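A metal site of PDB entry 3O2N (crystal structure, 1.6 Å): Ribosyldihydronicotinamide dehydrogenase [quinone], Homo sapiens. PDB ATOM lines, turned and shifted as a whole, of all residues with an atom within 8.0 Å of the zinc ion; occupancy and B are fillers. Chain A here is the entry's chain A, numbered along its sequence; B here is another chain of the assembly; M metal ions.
The zinc ion is bound by a ring nitrogen (ND1) of His 177, at 2.0 Å. A ring nitrogen (ND1) of His 173 binds the zinc ion (2.1 Å). The side-chain sulfur (SG) of Cys 222 binds the zinc ion, at 2.2 Å. The backbone carbonyl oxygen (O) of Cys 222 binds the zinc ion (2.2 Å). The zinc ion has four donor atoms within binding distance.
The backbone NH (N) of His 177 lies within hydrogen-bond range of the backbone carbonyl oxygen (O) of Gln 172, 2.6 Å away. O of Gln 172 sits close to SG of Cys 222 (3.6 Å). O of His 173 is in hydrogen-bond range of N of Phe 178, at 3.2 Å. The backbone carbonyl oxygen (O) of Val 160 of chain B sits at hydrogen-bond distance from a ring nitrogen (NE2) of His 173, 3.3 Å away. A ring nitrogen (NE2) of His 177 sits at hydrogen-bond distance from the side-chain carboxylate of Asp 133 (2.8 Å). The side-chain hydroxyl of Tyr 132 sits close to a ring nitrogen (NE2) of His 173.
Of the 21 residues printed, 3 come within 4 Å of the zinc ion.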
ATOM      1  N   TYR A 132      13.519 -21.417  18.829  1.00  0.00           N
ATOM      2  CA  TYR A 132      14.724 -21.640  18.053  1.00  0.00           C
ATOM      3  C   TYR A 132      14.580 -22.926  17.190  1.00  0.00           C
ATOM      4  O   TYR A 132      13.642 -23.002  16.357  1.00  0.00           O
ATOM      5  CB  TYR A 132      15.933 -21.680  19.010  1.00  0.00           C
ATOM      6  CG  TYR A 132      16.213 -20.270  19.490  1.00  0.00           C
ATOM      7  CD1 TYR A 132      16.513 -19.278  18.571  1.00  0.00           C
ATOM      8  CD2 TYR A 132      16.200 -19.948  20.865  1.00  0.00           C
ATOM      9  CE1 TYR A 132      16.803 -17.960  18.997  1.00  0.00           C
ATOM     10  CE2 TYR A 132      16.524 -18.611  21.335  1.00  0.00           C
ATOM     11  CZ  TYR A 132      16.802 -17.646  20.363  1.00  0.00           C
ATOM     12  OH  TYR A 132      17.083 -16.347  20.779  1.00  0.00           O
ATOM     13  N   ASP A 133      15.456 -23.929  17.342  1.00  0.00           N
ATOM     14  CA  ASP A 133      15.322 -25.174  16.548  1.00  0.00           C
ATOM     15  C   ASP A 133      13.954 -25.891  16.551  1.00  0.00           C
ATOM     16  O   ASP A 133      13.537 -26.524  15.515  1.00  0.00           O
ATOM     17  CB  ASP A 133      16.401 -26.144  16.971  1.00  0.00           C
ATOM     18  CG  ASP A 133      17.703 -25.751  16.420  1.00  0.00           C
ATOM     19  OD1 ASP A 133      17.767 -24.584  15.974  1.00  0.00           O
ATOM     20  OD2 ASP A 133      18.679 -26.567  16.406  1.00  0.00           O
ATOM     21  N   TRP A 169      21.314  -9.881  13.335  1.00  0.00           N
ATOM     22  CA  TRP A 169      21.059 -10.723  14.450  1.00  0.00           C
ATOM     23  C   TRP A 169      19.605 -10.668  14.998  1.00  0.00           C
ATOM     24  O   TRP A 169      18.957 -11.705  15.174  1.00  0.00           O
ATOM     25  CB  TRP A 169      22.139 -10.408  15.533  1.00  0.00           C
ATOM     26  CG  TRP A 169      21.928 -11.106  16.836  1.00  0.00           C
ATOM     27  CD1 TRP A 169      21.513 -10.525  18.052  1.00  0.00           C
ATOM     28  CD2 TRP A 169      22.254 -12.455  17.163  1.00  0.00           C
ATOM     29  NE1 TRP A 169      21.535 -11.426  19.054  1.00  0.00           N
ATOM     30  CE2 TRP A 169      22.005 -12.626  18.549  1.00  0.00           C
ATOM     31  CE3 TRP A 169      22.784 -13.530  16.420  1.00  0.00           C
ATOM     32  CZ2 TRP A 169      22.219 -13.844  19.206  1.00  0.00           C
ATOM     33  CZ3 TRP A 169      22.947 -14.735  17.062  1.00  0.00           C
ATOM     34  CH2 TRP A 169      22.723 -14.882  18.464  1.00  0.00           C
ATOM     35  N   LEU A 171      16.947  -9.862  13.536  1.00  0.00           N
ATOM     36  CA  LEU A 171      15.940 -10.323  12.541  1.00  0.00           C
ATOM     37  C   LEU A 171      16.149 -11.822  12.284  1.00  0.00           C
ATOM     38  O   LEU A 171      15.195 -12.546  12.359  1.00  0.00           O
ATOM     39  CB  LEU A 171      16.135  -9.565  11.255  1.00  0.00           C
ATOM     40  CG  LEU A 171      15.927  -8.026  11.438  1.00  0.00           C
ATOM     41  CD1 LEU A 171      16.364  -7.301  10.168  1.00  0.00           C
ATOM     42  CD2 LEU A 171      14.461  -7.726  11.750  1.00  0.00           C
ATOM     43  N   GLN A 172      17.359 -12.204  11.964  1.00  0.00           N
ATOM     44  CA  GLN A 172      17.568 -13.621  11.596  1.00  0.00           C
ATOM     45  C   GLN A 172      17.467 -14.522  12.777  1.00  0.00           C
ATOM     46  O   GLN A 172      16.787 -15.606  12.758  1.00  0.00           O
ATOM     47  CB  GLN A 172      18.894 -13.749  10.892  1.00  0.00           C
ATOM     48  CG  GLN A 172      18.930 -13.147   9.540  1.00  0.00           C
ATOM     49  CD  GLN A 172      20.145 -13.561   8.769  1.00  0.00           C
ATOM     50  OE1 GLN A 172      21.240 -13.864   9.359  1.00  0.00           O
ATOM     51  NE2 GLN A 172      20.048 -13.476   7.460  1.00  0.00           N
ATOM     52  N   HIS A 173      18.148 -14.132  13.887  1.00  0.00           N
ATOM     53  CA  HIS A 173      18.198 -14.951  15.039  1.00  0.00           C
ATOM     54  C   HIS A 173      17.094 -14.692  15.994  1.00  0.00           C
ATOM     55  O   HIS A 173      16.322 -15.585  16.331  1.00  0.00           O
ATOM     56  CB  HIS A 173      19.567 -14.832  15.752  1.00  0.00           C
ATOM     57  CG  HIS A 173      19.719 -15.769  16.923  1.00  0.00           C
ATOM     58  ND1 HIS A 173      20.000 -17.122  16.780  1.00  0.00           N
ATOM     59  CD2 HIS A 173      19.616 -15.580  18.267  1.00  0.00           C
ATOM     60  CE1 HIS A 173      20.033 -17.708  17.974  1.00  0.00           C
ATOM     61  NE2 HIS A 173      19.842 -16.783  18.897  1.00  0.00           N
ATOM     62  N   GLY A 174      16.934 -13.449  16.450  1.00  0.00           N
ATOM     63  CA  GLY A 174      15.920 -13.163  17.433  1.00  0.00           C
ATOM     64  C   GLY A 174      14.460 -13.324  16.958  1.00  0.00           C
ATOM     65  O   GLY A 174      13.595 -13.584  17.776  1.00  0.00           O
ATOM     66  N   THR A 175      14.289 -13.254  15.634  1.00  0.00           N
ATOM     67  CA  THR A 175      12.922 -13.359  15.122  1.00  0.00           C
ATOM     68  C   THR A 175      12.782 -14.686  14.320  1.00  0.00           C
ATOM     69  O   THR A 175      11.970 -15.519  14.773  1.00  0.00           O
ATOM     70  CB  THR A 175      12.543 -12.153  14.262  1.00  0.00           C
ATOM     71  OG1 THR A 175      12.774 -10.981  15.075  1.00  0.00           O
ATOM     72  CG2 THR A 175      11.029 -12.154  13.976  1.00  0.00           C
ATOM     73  N   LEU A 176      13.465 -14.794  13.210  1.00  0.00           N
ATOM     74  CA  LEU A 176      13.183 -15.965  12.204  1.00  0.00           C
ATOM     75  C   LEU A 176      13.626 -17.309  12.814  1.00  0.00           C
ATOM     76  O   LEU A 176      12.801 -18.187  13.041  1.00  0.00           O
ATOM     77  CB  LEU A 176      13.838 -15.747  10.857  1.00  0.00           C
ATOM     78  CG  LEU A 176      13.341 -14.415  10.148  1.00  0.00           C
ATOM     79  CD1 LEU A 176      14.123 -14.147   8.897  1.00  0.00           C
ATOM     80  CD2 LEU A 176      11.867 -14.457   9.931  1.00  0.00           C
ATOM     81  N   HIS A 177      14.877 -17.362  13.255  1.00  0.00           N
ATOM     82  CA  HIS A 177      15.326 -18.612  13.996  1.00  0.00           C
ATOM     83  C   HIS A 177      14.459 -18.882  15.195  1.00  0.00           C
ATOM     84  O   HIS A 177      14.031 -20.017  15.486  1.00  0.00           O
ATOM     85  CB  HIS A 177      16.817 -18.512  14.345  1.00  0.00           C
ATOM     86  CG  HIS A 177      17.410 -19.786  14.856  1.00  0.00           C
ATOM     87  ND1 HIS A 177      18.742 -19.852  15.203  1.00  0.00           N
ATOM     88  CD2 HIS A 177      16.907 -21.038  14.982  1.00  0.00           C
ATOM     89  CE1 HIS A 177      19.025 -21.087  15.598  1.00  0.00           C
ATOM     90  NE2 HIS A 177      17.938 -21.844  15.456  1.00  0.00           N
ATOM     91  N   PHE A 178      14.155 -17.879  16.029  1.00  0.00           N
ATOM     92  CA  PHE A 178      13.318 -18.082  17.140  1.00  0.00           C
ATOM     93  C   PHE A 178      12.043 -18.795  16.818  1.00  0.00           C
ATOM     94  O   PHE A 178      11.553 -19.573  17.582  1.00  0.00           O
ATOM     95  CB  PHE A 178      13.101 -16.729  17.977  1.00  0.00           C
ATOM     96  CG  PHE A 178      12.461 -16.920  19.257  1.00  0.00           C
ATOM     97  CD1 PHE A 178      13.237 -17.109  20.439  1.00  0.00           C
ATOM     98  CD2 PHE A 178      11.109 -16.799  19.400  1.00  0.00           C
ATOM     99  CE1 PHE A 178      12.575 -17.251  21.681  1.00  0.00           C
ATOM    100  CE2 PHE A 178      10.466 -16.938  20.556  1.00  0.00           C
ATOM    101  CZ  PHE A 178      11.205 -17.204  21.770  1.00  0.00           C
ATOM    102  N   PHE A 181      12.166 -21.053  11.758  1.00  0.00           N
ATOM    103  CA  PHE A 181      12.661 -21.001  10.408  1.00  0.00           C
ATOM    104  C   PHE A 181      14.112 -21.410  10.219  1.00  0.00           C
ATOM    105  O   PHE A 181      14.970 -21.110  11.045  1.00  0.00           O
ATOM    106  CB  PHE A 181      12.582 -19.574   9.761  1.00  0.00           C
ATOM    107  CG  PHE A 181      11.192 -19.024   9.525  1.00  0.00           C
ATOM    108  CD1 PHE A 181      10.460 -19.373   8.388  1.00  0.00           C
ATOM    109  CD2 PHE A 181      10.693 -18.019  10.336  1.00  0.00           C
ATOM    110  CE1 PHE A 181       9.181 -18.814   8.114  1.00  0.00           C
ATOM    111  CE2 PHE A 181       9.404 -17.423  10.084  1.00  0.00           C
ATOM    112  CZ  PHE A 181       8.686 -17.846   8.915  1.00  0.00           C
ATOM    113  N   VAL A 183      17.009 -20.259   8.021  1.00  0.00           N
ATOM    114  CA  VAL A 183      17.233 -19.003   7.433  1.00  0.00           C
ATOM    115  C   VAL A 183      18.173 -19.173   6.295  1.00  0.00           C
ATOM    116  O   VAL A 183      19.318 -19.615   6.450  1.00  0.00           O
ATOM    117  CB  VAL A 183      17.891 -17.978   8.504  1.00  0.00           C
ATOM    118  CG1 VAL A 183      18.256 -16.647   7.867  1.00  0.00           C
ATOM    119  CG2 VAL A 183      17.077 -17.932   9.688  1.00  0.00           C
ATOM    120  N   ILE A 220      21.890 -20.928   6.314  1.00  0.00           N
ATOM    121  CA  ILE A 220      23.024 -20.542   7.141  1.00  0.00           C
ATOM    122  C   ILE A 220      22.949 -21.256   8.528  1.00  0.00           C
ATOM    123  O   ILE A 220      21.893 -21.685   9.005  1.00  0.00           O
ATOM    124  CB  ILE A 220      23.086 -19.056   7.285  1.00  0.00           C
ATOM    125  CG1 ILE A 220      21.881 -18.551   8.096  1.00  0.00           C
ATOM    126  CG2 ILE A 220      23.261 -18.412   5.942  1.00  0.00           C
ATOM    127  CD1 ILE A 220      22.195 -17.236   8.867  1.00  0.00           C
ATOM    128  N   PRO A 221      24.133 -21.427   9.203  1.00  0.00           N
ATOM    129  CA  PRO A 221      24.036 -21.925  10.593  1.00  0.00           C
ATOM    130  C   PRO A 221      23.719 -20.655  11.412  1.00  0.00           C
ATOM    131  O   PRO A 221      24.561 -19.752  11.453  1.00  0.00           O
ATOM    132  CB  PRO A 221      25.474 -22.418  10.905  1.00  0.00           C
ATOM    133  CG  PRO A 221      26.368 -21.661   9.947  1.00  0.00           C
ATOM    134  CD  PRO A 221      25.506 -21.364   8.699  1.00  0.00           C
ATOM    135  N   CYS A 222      22.507 -20.550  11.998  1.00  0.00           N
ATOM    136  CA  CYS A 222      22.036 -19.217  12.494  1.00  0.00           C
ATOM    137  C   CYS A 222      22.509 -19.110  13.936  1.00  0.00           C
ATOM    138  O   CYS A 222      21.785 -19.438  14.909  1.00  0.00           O
ATOM    139  CB  CYS A 222      20.506 -19.090  12.380  1.00  0.00           C
ATOM    140  SG  CYS A 222      19.923 -17.439  13.046  1.00  0.00           S
ATOM    141  N   THR A 223      23.778 -18.753  14.073  1.00  0.00           N
ATOM    142  CA  THR A 223      24.384 -18.821  15.391  1.00  0.00           C
ATOM    143  C   THR A 223      25.093 -17.514  15.745  1.00  0.00           C
ATOM    144  O   THR A 223      25.421 -16.705  14.860  1.00  0.00           O
ATOM    145  CB  THR A 223      25.456 -20.003  15.479  1.00  0.00           C
ATOM    146  OG1 THR A 223      26.489 -19.755  14.510  1.00  0.00           O
ATOM    147  CG2 THR A 223      24.846 -21.397  15.358  1.00  0.00           C
ATOM    148  N   ALA A 224      25.383 -17.320  17.035  1.00  0.00           N
ATOM    149  CA  ALA A 224      26.222 -16.184  17.434  1.00  0.00           C
ATOM    150  C   ALA A 224      27.559 -16.172  16.687  1.00  0.00           C
ATOM    151  O   ALA A 224      28.004 -15.119  16.212  1.00  0.00           O
ATOM    152  CB  ALA A 224      26.395 -16.139  19.032  1.00  0.00           C
ATOM    153  N   TRP A 226      28.137 -17.456  13.602  1.00  0.00           N
ATOM    154  CA  TRP A 226      27.868 -16.944  12.244  1.00  0.00           C
ATOM    155  C   TRP A 226      27.811 -15.385  12.173  1.00  0.00           C
ATOM    156  O   TRP A 226      28.342 -14.789  11.238  1.00  0.00           O
ATOM    157  CB  TRP A 226      26.599 -17.604  11.570  1.00  0.00           C
ATOM    158  CG  TRP A 226      26.437 -17.269  10.055  1.00  0.00           C
ATOM    159  CD1 TRP A 226      26.836 -18.043   8.995  1.00  0.00           C
ATOM    160  CD2 TRP A 226      25.837 -16.072   9.465  1.00  0.00           C
ATOM    161  NE1 TRP A 226      26.555 -17.411   7.789  1.00  0.00           N
ATOM    162  CE2 TRP A 226      25.915 -16.203   8.049  1.00  0.00           C
ATOM    163  CE3 TRP A 226      25.224 -14.916   9.991  1.00  0.00           C
ATOM    164  CZ2 TRP A 226      25.440 -15.212   7.149  1.00  0.00           C
ATOM    165  CZ3 TRP A 226      24.750 -13.906   9.090  1.00  0.00           C
ATOM    166  CH2 TRP A 226      24.840 -14.084   7.684  1.00  0.00           C
ATOM    167  N   HIS A 227      27.145 -14.740  13.148  1.00  0.00           N
ATOM    168  CA  HIS A 227      26.962 -13.268  13.078  1.00  0.00           C
ATOM    169  C   HIS A 227      28.158 -12.446  13.585  1.00  0.00           C
ATOM    170  O   HIS A 227      28.430 -11.360  13.069  1.00  0.00           O
ATOM    171  CB  HIS A 227      25.672 -12.809  13.797  1.00  0.00           C
ATOM    172  CG  HIS A 227      24.409 -13.343  13.172  1.00  0.00           C
ATOM    173  ND1 HIS A 227      23.949 -14.641  13.383  1.00  0.00           N
ATOM    174  CD2 HIS A 227      23.484 -12.723  12.401  1.00  0.00           C
ATOM    175  CE1 HIS A 227      22.804 -14.796  12.717  1.00  0.00           C
ATOM    176  NE2 HIS A 227      22.506 -13.650  12.109  1.00  0.00           N
ATOM    177  N   VAL B 160      20.795 -18.789  25.493  1.00  0.00           N
ATOM    178  CA  VAL B 160      20.059 -19.065  24.214  1.00  0.00           C
ATOM    179  C   VAL B 160      19.978 -17.863  23.282  1.00  0.00           C
ATOM    180  O   VAL B 160      20.111 -17.930  22.014  1.00  0.00           O
ATOM    181  CB  VAL B 160      18.543 -19.477  24.457  1.00  0.00           C
ATOM    182  CG1 VAL B 160      18.389 -20.970  24.321  1.00  0.00           C
ATOM    183  CG2 VAL B 160      18.015 -18.995  25.791  1.00  0.00           C
HETATM  184 ZN    ZN M   1      19.919 -18.257  15.058  1.00  0.00          ZN
